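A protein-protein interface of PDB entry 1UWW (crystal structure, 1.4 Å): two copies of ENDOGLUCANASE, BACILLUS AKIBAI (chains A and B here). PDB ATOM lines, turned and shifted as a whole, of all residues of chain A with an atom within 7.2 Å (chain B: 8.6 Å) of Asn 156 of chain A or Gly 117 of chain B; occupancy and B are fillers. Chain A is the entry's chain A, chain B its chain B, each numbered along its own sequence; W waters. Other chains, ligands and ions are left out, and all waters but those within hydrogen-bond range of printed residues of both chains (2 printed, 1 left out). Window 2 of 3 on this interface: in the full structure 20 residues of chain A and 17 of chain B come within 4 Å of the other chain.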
ATOM      1  N   ARG A  83      20.885 -28.073  22.910  1.00  0.00           N
ATOM      2  CA  ARG A  83      19.482 -27.713  22.933  1.00  0.00           C
ATOM      3  C   ARG A  83      18.639 -28.555  21.995  1.00  0.00           C
ATOM      4  O   ARG A  83      17.489 -28.881  22.277  1.00  0.00           O
ATOM      5  CB  ARG A  83      19.294 -26.240  22.567  1.00  0.00           C
ATOM      6  CG  ARG A  83      17.846 -25.744  22.572  1.00  0.00           C
ATOM      7  CD  ARG A  83      17.716 -24.283  22.341  1.00  0.00           C
ATOM      8  NE  ARG A  83      18.256 -23.903  21.031  1.00  0.00           N
ATOM      9  CZ  ARG A  83      18.615 -22.678  20.684  1.00  0.00           C
ATOM     10  NH1 ARG A  83      18.516 -21.660  21.516  1.00  0.00           N
ATOM     11  NH2 ARG A  83      19.109 -22.457  19.467  1.00  0.00           N
ATOM     12  N   PRO A 113      29.174 -22.791  26.841  1.00  0.00           N
ATOM     13  CA  PRO A 113      29.721 -23.223  25.543  1.00  0.00           C
ATOM     14  C   PRO A 113      31.088 -22.567  25.277  1.00  0.00           C
ATOM     15  O   PRO A 113      31.163 -21.351  25.280  1.00  0.00           O
ATOM     16  CB  PRO A 113      28.703 -22.708  24.518  1.00  0.00           C
ATOM     17  CG  PRO A 113      27.928 -21.637  25.242  1.00  0.00           C
ATOM     18  CD  PRO A 113      27.972 -21.961  26.684  1.00  0.00           C
ATOM     19  N   THR A 115      32.430 -22.072  22.557  1.00  0.00           N
ATOM     20  CA  THR A 115      32.281 -21.205  21.380  1.00  0.00           C
ATOM     21  C   THR A 115      31.589 -19.869  21.654  1.00  0.00           C
ATOM     22  O   THR A 115      31.564 -19.006  20.762  1.00  0.00           O
ATOM     23  CB  THR A 115      31.513 -21.916  20.256  1.00  0.00           C
ATOM     24  OG1 THR A 115      30.229 -22.350  20.736  1.00  0.00           O
ATOM     25  CG2 THR A 115      32.220 -23.166  19.813  1.00  0.00           C
ATOM     26  N   ASN A 116      30.967 -19.700  22.828  1.00  0.00           N
ATOM     27  CA  ASN A 116      30.431 -18.394  23.242  1.00  0.00           C
ATOM     28  C   ASN A 116      30.941 -17.897  24.580  1.00  0.00           C
ATOM     29  O   ASN A 116      30.163 -17.571  25.482  1.00  0.00           O
ATOM     30  CB  ASN A 116      28.889 -18.361  23.264  1.00  0.00           C
ATOM     31  CG  ASN A 116      28.337 -16.938  23.062  1.00  0.00           C
ATOM     32  OD1 ASN A 116      28.225 -16.462  21.919  1.00  0.00           O
ATOM     33  ND2 ASN A 116      28.027 -16.243  24.165  1.00  0.00           N
ATOM     34  N   TRP A 119      29.838 -18.692  28.601  1.00  0.00           N
ATOM     35  CA  TRP A 119      28.738 -18.123  29.385  1.00  0.00           C
ATOM     36  C   TRP A 119      27.630 -17.687  28.468  1.00  0.00           C
ATOM     37  O   TRP A 119      27.777 -16.725  27.704  1.00  0.00           O
ATOM     38  CB  TRP A 119      29.184 -16.906  30.227  1.00  0.00           C
ATOM     39  CG  TRP A 119      28.153 -16.495  31.215  1.00  0.00           C
ATOM     40  CD1 TRP A 119      27.068 -15.682  31.004  1.00  0.00           C
ATOM     41  CD2 TRP A 119      28.097 -16.888  32.572  1.00  0.00           C
ATOM     42  NE1 TRP A 119      26.332 -15.589  32.157  1.00  0.00           N
ATOM     43  CE2 TRP A 119      26.945 -16.305  33.147  1.00  0.00           C
ATOM     44  CE3 TRP A 119      28.901 -17.694  33.374  1.00  0.00           C
ATOM     45  CZ2 TRP A 119      26.601 -16.477  34.495  1.00  0.00           C
ATOM     46  CZ3 TRP A 119      28.559 -17.863  34.700  1.00  0.00           C
ATOM     47  CH2 TRP A 119      27.417 -17.264  35.248  1.00  0.00           C
ATOM     48  N   VAL A 120      26.512 -18.404  28.523  1.00  0.00           N
ATOM     49  CA  VAL A 120      25.242 -17.936  27.996  1.00  0.00           C
ATOM     50  C   VAL A 120      24.204 -18.187  29.077  1.00  0.00           C
ATOM     51  O   VAL A 120      24.303 -19.122  29.851  1.00  0.00           O
ATOM     52  CB  VAL A 120      24.838 -18.611  26.667  1.00  0.00           C
ATOM     53  CG1 VAL A 120      25.863 -18.360  25.577  1.00  0.00           C
ATOM     54  CG2 VAL A 120      24.571 -20.086  26.834  1.00  0.00           C
ATOM     55  N   ASP A 153      14.909 -19.012  23.450  1.00  0.00           N
ATOM     56  CA  ASP A 153      15.191 -17.577  23.411  1.00  0.00           C
ATOM     57  C   ASP A 153      16.656 -17.210  23.593  1.00  0.00           C
ATOM     58  O   ASP A 153      16.996 -16.015  23.551  1.00  0.00           O
ATOM     59  CB  ASP A 153      14.286 -16.852  24.410  1.00  0.00           C
ATOM     60  CG  ASP A 153      12.821 -16.828  23.946  1.00  0.00           C
ATOM     61  OD1 ASP A 153      12.572 -17.149  22.755  1.00  0.00           O
ATOM     62  OD2 ASP A 153      11.859 -16.541  24.679  1.00  0.00           O
ATOM     63  N   ILE A 154      17.551 -18.185  23.732  1.00  0.00           N
ATOM     64  CA  ILE A 154      18.988 -17.903  23.749  1.00  0.00           C
ATOM     65  C   ILE A 154      19.460 -17.799  22.314  1.00  0.00           C
ATOM     66  O   ILE A 154      19.601 -18.797  21.628  1.00  0.00           O
ATOM     67  CB  ILE A 154      19.772 -19.005  24.530  1.00  0.00           C
ATOM     68  CG1 ILE A 154      19.289 -19.096  25.984  1.00  0.00           C
ATOM     69  CG2 ILE A 154      21.279 -18.724  24.546  1.00  0.00           C
ATOM     70  CD1 ILE A 154      19.819 -20.281  26.757  1.00  0.00           C
ATOM     71  N   THR A 155      19.752 -16.580  21.872  1.00  0.00           N
ATOM     72  CA  THR A 155      20.172 -16.368  20.489  1.00  0.00           C
ATOM     73  C   THR A 155      21.631 -16.631  20.244  1.00  0.00           C
ATOM     74  O   THR A 155      22.002 -16.829  19.087  1.00  0.00           O
ATOM     75  CB  THR A 155      19.864 -14.956  20.007  1.00  0.00           C
ATOM     76  OG1 THR A 155      20.575 -14.000  20.808  1.00  0.00           O
ATOM     77  CG2 THR A 155      18.377 -14.643  20.162  1.00  0.00           C
ATOM     78  N   ASN A 156      22.459 -16.666  21.285  1.00  0.00           N
ATOM     79  CA  ASN A 156      23.897 -16.891  21.098  1.00  0.00           C
ATOM     80  C   ASN A 156      24.298 -18.350  21.180  1.00  0.00           C
ATOM     81  O   ASN A 156      25.472 -18.679  21.377  1.00  0.00           O
ATOM     82  CB  ASN A 156      24.707 -16.079  22.097  1.00  0.00           C
ATOM     83  CG  ASN A 156      25.121 -14.739  21.546  1.00  0.00           C
ATOM     84  OD1 ASN A 156      25.509 -14.617  20.372  1.00  0.00           O
ATOM     85  ND2 ASN A 156      25.064 -13.735  22.387  1.00  0.00           N
ATOM     86  N   ILE A 157      23.319 -19.237  21.050  1.00  0.00           N
ATOM     87  CA  ILE A 157      23.614 -20.631  20.761  1.00  0.00           C
ATOM     88  C   ILE A 157      22.784 -21.038  19.563  1.00  0.00           C
ATOM     89  O   ILE A 157      21.844 -20.367  19.184  1.00  0.00           O
ATOM     90  CB  ILE A 157      23.343 -21.596  21.961  1.00  0.00           C
ATOM     91  CG1 ILE A 157      21.850 -21.665  22.287  1.00  0.00           C
ATOM     92  CG2 ILE A 157      24.198 -21.223  23.196  1.00  0.00           C
ATOM     93  CD1 ILE A 157      21.501 -22.557  23.444  1.00  0.00           C
ATOM     94  N   GLN A 158      23.177 -22.156  18.977  1.00  0.00           N
ATOM     95  CA  GLN A 158      22.415 -22.815  17.927  1.00  0.00           C
ATOM     96  C   GLN A 158      21.983 -24.177  18.425  1.00  0.00           C
ATOM     97  O   GLN A 158      22.383 -24.616  19.506  1.00  0.00           O
ATOM     98  CB  GLN A 158      23.312 -22.961  16.722  1.00  0.00           C
ATOM     99  CG  GLN A 158      23.706 -21.604  16.180  1.00  0.00           C
ATOM    100  CD  GLN A 158      24.754 -21.660  15.142  1.00  0.00           C
ATOM    101  OE1 GLN A 158      25.692 -22.469  15.212  1.00  0.00           O
ATOM    102  NE2 GLN A 158      24.631 -20.765  14.177  1.00  0.00           N
ATOM    103  N   THR A 161      24.993 -26.391  19.119  1.00  0.00           N
ATOM    104  CA  THR A 161      26.107 -25.864  19.924  1.00  0.00           C
ATOM    105  C   THR A 161      26.383 -26.740  21.150  1.00  0.00           C
ATOM    106  O   THR A 161      25.463 -27.014  21.934  1.00  0.00           O
ATOM    107  CB  THR A 161      25.775 -24.473  20.417  1.00  0.00           C
ATOM    108  OG1 THR A 161      25.567 -23.607  19.299  1.00  0.00           O
ATOM    109  CG2 THR A 161      26.938 -23.867  21.226  1.00  0.00           C
ATOM    110  N   LEU A 163      27.203 -27.272  24.720  1.00  0.00           N
ATOM    111  CA  LEU A 163      27.002 -26.395  25.860  1.00  0.00           C
ATOM    112  C   LEU A 163      27.953 -26.695  27.023  1.00  0.00           C
ATOM    113  O   LEU A 163      28.119 -25.840  27.904  1.00  0.00           O
ATOM    114  CB  LEU A 163      25.536 -26.478  26.304  1.00  0.00           C
ATOM    115  CG  LEU A 163      24.523 -26.066  25.225  1.00  0.00           C
ATOM    116  CD1 LEU A 163      23.091 -26.378  25.681  1.00  0.00           C
ATOM    117  CD2 LEU A 163      24.686 -24.603  24.881  1.00  0.00           C
ATOM    118  N   PHE B 111      22.640  -5.494  26.719  1.00  0.00           N
ATOM    119  CA  PHE B 111      23.328  -4.721  25.664  1.00  0.00           C
ATOM    120  C   PHE B 111      23.378  -5.535  24.400  1.00  0.00           C
ATOM    121  O   PHE B 111      23.233  -6.751  24.438  1.00  0.00           O
ATOM    122  CB  PHE B 111      24.745  -4.350  26.058  1.00  0.00           C
ATOM    123  CG  PHE B 111      24.843  -3.543  27.304  1.00  0.00           C
ATOM    124  CD1 PHE B 111      24.569  -2.187  27.296  1.00  0.00           C
ATOM    125  CD2 PHE B 111      25.261  -4.137  28.462  1.00  0.00           C
ATOM    126  CE1 PHE B 111      24.681  -1.437  28.476  1.00  0.00           C
ATOM    127  CE2 PHE B 111      25.397  -3.405  29.638  1.00  0.00           C
ATOM    128  CZ  PHE B 111      25.113  -2.033  29.634  1.00  0.00           C
ATOM    129  N   GLN B 112      23.599  -4.882  23.263  1.00  0.00           N
ATOM    130  CA  GLN B 112      23.627  -5.605  21.982  1.00  0.00           C
ATOM    131  C   GLN B 112      24.912  -5.359  21.199  1.00  0.00           C
ATOM    132  O   GLN B 112      24.856  -4.830  20.080  1.00  0.00           O
ATOM    133  CB  GLN B 112      22.396  -5.288  21.152  1.00  0.00           C
ATOM    134  CG  GLN B 112      21.075  -5.567  21.851  1.00  0.00           C
ATOM    135  CD  GLN B 112      19.940  -5.668  20.861  1.00  0.00           C
ATOM    136  OE1 GLN B 112      19.297  -4.671  20.550  1.00  0.00           O
ATOM    137  NE2 GLN B 112      19.736  -6.862  20.290  1.00  0.00           N
ATOM    138  N   PRO B 113      26.056  -5.735  21.766  1.00  0.00           N
ATOM    139  CA  PRO B 113      27.333  -5.514  21.072  1.00  0.00           C
ATOM    140  C   PRO B 113      27.384  -6.320  19.766  1.00  0.00           C
ATOM    141  O   PRO B 113      27.205  -7.534  19.844  1.00  0.00           O
ATOM    142  CB  PRO B 113      28.374  -6.002  22.067  1.00  0.00           C
ATOM    143  CG  PRO B 113      27.653  -6.701  23.163  1.00  0.00           C
ATOM    144  CD  PRO B 113      26.232  -6.444  23.042  1.00  0.00           C
ATOM    145  N   PRO B 114      27.646  -5.703  18.622  1.00  0.00           N
ATOM    146  CA  PRO B 114      27.789  -6.493  17.383  1.00  0.00           C
ATOM    147  C   PRO B 114      28.860  -7.578  17.472  1.00  0.00           C
ATOM    148  O   PRO B 114      28.656  -8.626  16.864  1.00  0.00           O
ATOM    149  CB  PRO B 114      28.161  -5.447  16.354  1.00  0.00           C
ATOM    150  CG  PRO B 114      27.485  -4.226  16.872  1.00  0.00           C
ATOM    151  CD  PRO B 114      27.726  -4.261  18.356  1.00  0.00           C
ATOM    152  N   THR B 115      29.932  -7.379  18.233  1.00  0.00           N
ATOM    153  CA  THR B 115      30.947  -8.433  18.403  1.00  0.00           C
ATOM    154  C   THR B 115      30.505  -9.606  19.268  1.00  0.00           C
ATOM    155  O   THR B 115      31.202 -10.598  19.343  1.00  0.00           O
ATOM    156  CB  THR B 115      32.221  -7.870  18.990  1.00  0.00           C
ATOM    157  OG1 THR B 115      31.911  -7.132  20.185  1.00  0.00           O
ATOM    158  CG2 THR B 115      32.873  -6.900  18.017  1.00  0.00           C
ATOM    159  N   ASN B 116      29.384  -9.488  19.968  1.00  0.00           N
ATOM    160  CA  ASN B 116      28.851 -10.575  20.793  1.00  0.00           C
ATOM    161  C   ASN B 116      27.463 -11.025  20.315  1.00  0.00           C
ATOM    162  O   ASN B 116      26.547 -11.228  21.109  1.00  0.00           O
ATOM    163  CB  ASN B 116      28.753 -10.099  22.244  1.00  0.00           C
ATOM    164  CG  ASN B 116      30.094  -9.799  22.875  1.00  0.00           C
ATOM    165  OD1 ASN B 116      30.739  -8.787  22.587  1.00  0.00           O
ATOM    166  ND2 ASN B 116      30.518 -10.680  23.780  1.00  0.00           N
ATOM    167  N   GLY B 117      27.276 -11.123  19.012  1.00  0.00           N
ATOM    168  CA  GLY B 117      26.016 -11.613  18.484  1.00  0.00           C
ATOM    169  C   GLY B 117      24.795 -10.763  18.823  1.00  0.00           C
ATOM    170  O   GLY B 117      23.660 -11.230  18.814  1.00  0.00           O
ATOM    171  N   TYR B 118      25.017  -9.490  19.123  1.00  0.00           N
ATOM    172  CA  TYR B 118      23.949  -8.544  19.460  1.00  0.00           C
ATOM    173  C   TYR B 118      23.200  -8.916  20.751  1.00  0.00           C
ATOM    174  O   TYR B 118      22.050  -8.543  20.912  1.00  0.00           O
ATOM    175  CB  TYR B 118      22.976  -8.329  18.271  1.00  0.00           C
ATOM    176  CG  TYR B 118      23.651  -7.923  16.964  1.00  0.00           C
ATOM    177  CD1 TYR B 118      24.005  -6.599  16.708  1.00  0.00           C
ATOM    178  CD2 TYR B 118      23.969  -8.868  16.003  1.00  0.00           C
ATOM    179  CE1 TYR B 118      24.612  -6.227  15.534  1.00  0.00           C
ATOM    180  CE2 TYR B 118      24.622  -8.518  14.845  1.00  0.00           C
ATOM    181  CZ  TYR B 118      24.922  -7.188  14.600  1.00  0.00           C
ATOM    182  OH  TYR B 118      25.570  -6.770  13.450  1.00  0.00           O
ATOM    183  N   TRP B 119      23.857  -9.604  21.688  1.00  0.00           N
ATOM    184  CA  TRP B 119      23.202  -9.887  22.979  1.00  0.00           C
ATOM    185  C   TRP B 119      24.172 -10.260  24.079  1.00  0.00           C
ATOM    186  O   TRP B 119      24.859 -11.296  23.998  1.00  0.00           O
ATOM    187  CB  TRP B 119      22.208 -11.050  22.822  1.00  0.00           C
ATOM    188  CG  TRP B 119      21.297 -11.241  23.993  1.00  0.00           C
ATOM    189  CD1 TRP B 119      21.569 -11.921  25.154  1.00  0.00           C
ATOM    190  CD2 TRP B 119      19.971 -10.738  24.121  1.00  0.00           C
ATOM    191  NE1 TRP B 119      20.484 -11.853  25.993  1.00  0.00           N
ATOM    192  CE2 TRP B 119      19.481 -11.141  25.390  1.00  0.00           C
ATOM    193  CE3 TRP B 119      19.139  -9.960  23.290  1.00  0.00           C
ATOM    194  CZ2 TRP B 119      18.186 -10.818  25.835  1.00  0.00           C
ATOM    195  CZ3 TRP B 119      17.861  -9.639  23.732  1.00  0.00           C
ATOM    196  CH2 TRP B 119      17.402 -10.069  25.001  1.00  0.00           C
ATOM    197  N   VAL B 120      24.214  -9.424  25.107  1.00  0.00           N
ATOM    198  CA  VAL B 120      24.814  -9.799  26.394  1.00  0.00           C
ATOM    199  C   VAL B 120      23.885  -9.279  27.470  1.00  0.00           C
ATOM    200  O   VAL B 120      23.287  -8.241  27.314  1.00  0.00           O
ATOM    201  CB  VAL B 120      26.259  -9.274  26.603  1.00  0.00           C
ATOM    202  CG1 VAL B 120      27.203  -9.782  25.519  1.00  0.00           C
ATOM    203  CG2 VAL B 120      26.312  -7.782  26.688  1.00  0.00           C
ATOM    204  N   GLN B 121      23.771 -10.001  28.559  1.00  0.00           N
ATOM    205  CA  GLN B 121      22.858  -9.646  29.639  1.00  0.00           C
ATOM    206  C   GLN B 121      23.594  -9.541  30.946  1.00  0.00           C
ATOM    207  O   GLN B 121      24.439 -10.380  31.272  1.00  0.00           O
ATOM    208  CB  GLN B 121      21.778 -10.712  29.736  1.00  0.00           C
ATOM    209  CG  GLN B 121      20.557 -10.325  30.582  1.00  0.00           C
ATOM    210  CD  GLN B 121      19.383 -11.302  30.413  1.00  0.00           C
ATOM    211  OE1 GLN B 121      18.534 -11.440  31.311  1.00  0.00           O
ATOM    212  NE2 GLN B 121      19.325 -11.955  29.267  1.00  0.00           N
ATOM    213  N   ASN B 156      31.616 -11.553  29.023  1.00  0.00           N
ATOM    214  CA  ASN B 156      31.738 -11.717  27.580  1.00  0.00           C
ATOM    215  C   ASN B 156      32.178 -10.464  26.837  1.00  0.00           C
ATOM    216  O   ASN B 156      32.552 -10.550  25.662  1.00  0.00           O
ATOM    217  CB  ASN B 156      30.464 -12.353  27.004  1.00  0.00           C
ATOM    218  CG  ASN B 156      30.426 -13.860  27.256  1.00  0.00           C
ATOM    219  OD1 ASN B 156      31.459 -14.464  27.552  1.00  0.00           O
ATOM    220  ND2 ASN B 156      29.269 -14.462  27.143  1.00  0.00           N
ATOM    221  N   ARG B 164      26.655  -0.565  21.677  1.00  0.00           N
ATOM    222  CA  ARG B 164      25.679  -0.112  20.663  1.00  0.00           C
ATOM    223  C   ARG B 164      24.389   0.454  21.261  1.00  0.00           C
ATOM    224  O   ARG B 164      23.979   1.564  20.956  1.00  0.00           O
ATOM    225  CB  ARG B 164      25.379  -1.197  19.631  1.00  0.00           C
ATOM    226  CG  ARG B 164      24.561  -0.644  18.459  1.00  0.00           C
ATOM    227  CD  ARG B 164      24.078  -1.693  17.512  1.00  0.00           C
ATOM    228  NE  ARG B 164      22.977  -2.434  18.092  1.00  0.00           N
ATOM    229  CZ  ARG B 164      22.210  -3.292  17.449  1.00  0.00           C
ATOM    230  NH1 ARG B 164      22.494  -3.577  16.176  1.00  0.00           N
ATOM    231  NH2 ARG B 164      21.189  -3.874  18.059  1.00  0.00           N
HETATM  232  O   HOH W   1      21.047 -11.570  19.501  1.00  0.00           O
HETATM  233  O   HOH W   2      19.548 -14.128  23.612  1.00  0.00           O
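O of Trp 119 of chain A is in hydrogen-bond range of ND2 of Asn 156 of chain B (2.8 Å).
ND2 of Asn 156 of chain A lies within hydrogen-bond range of O of Asn 116 of chain B, 3.2 Å away.
O of Trp 119 of chain B is in hydrogen-bond range of ND2 of Asn 156 of chain A (2.9 Å).
OG1 of Thr 115 of chain B sits at hydrogen-bond distance from OD1 of Asn 116 of chain B (3.1 Å).
The side-chain amide nitrogen (ND2) of Asn 116 of chain B sits at hydrogen-bond distance from the backbone carbonyl oxygen (O) of Asn 156 of chain B, 2.8 Å away.
The indole nitrogen (NE1) of Trp 119 of chain B sits close to the side-chain amide nitrogen (NE2) of Gln 121 of chain B (3.5 Å).
Asn 116 of chain A touches Asn 156 of chain B (O to ND2, 3.6 Å).
CB of Trp 119 of chain B touches OG1 of Thr 155 of chain A, at 3.9 Å.
CA of Gly 117 of chain B touches OD1 of Asn 156 of chain A (3.6 Å).
Pro 113 of chain A touches none of the printed residues of chain B.
Of the printed residues of chain B, Asn 116 of chain A touches Asn 156 (3.6 Å).
Of the printed residues of chain B, Trp 119 of chain A touches Asn 156.
Ile 154 of chain A touches none of the printed residues of chain B.
Printed residues of chain B within 4 Å of Thr 155 of chain A: Trp 119.
Of the printed residues of chain B, Asn 156 of chain A touches Asn 116, Gly 117 and Trp 119.
Of the printed residues of chain A, Gly 117 of chain B touches Asn 156.
Printed residues of chain A within 4 Å of Asn 156 of chain B: Asn 116 (3.6 Å) and Trp 119 (2.8 Å).
The nearest residue of chain B that does not touch Asn 156 of chain A is Val 120 of chain B (5.2 Å).
The nearest printed residue of chain A that does not touch Asn 116 of chain B is Asn 116 of chain A (5.6 Å).
Hydrophobic or aromatic side chains of chain A within 4 Å of the printed part of chain B: Trp 119.
Printed residues of chain B that touch a printed residue of chain A: Asn 116, Gly 117, Trp 119 and Asn 156.
Hydrophobic or aromatic side chains of chain B within 4 Å of the printed part of chain A: Trp 119.
Asn 116 of chain A touches Asn 156 of chain B, and with the chains exchanged Asn 156 of chain A touches Asn 116 of chain B.
Trp 119 of chain A touches Asn 156 of chain B, and with the chains exchanged Asn 156 of chain A touches Trp 119 of chain B.
Of the 6 pairs that touch across the chains among the printed residues, 4 have their exchanged pair printed and touching as well.
Water W1 lies within hydrogen-bond range of O of Gly 117 of chain B (2.7 Å), OG1 of Thr 155 of chain A (2.8 Å) and O of Tyr 118 of chain B (3.5 Å).
Water W2 lies within hydrogen-bond range of the side-chain hydroxyl (OG1) of Thr 155 of chain A (3.0 Å), the backbone carbonyl oxygen (O) of Asp 153 of chain A (3.2 Å) and the indole nitrogen (NE1) of Trp 119 of chain B (3.4 Å).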
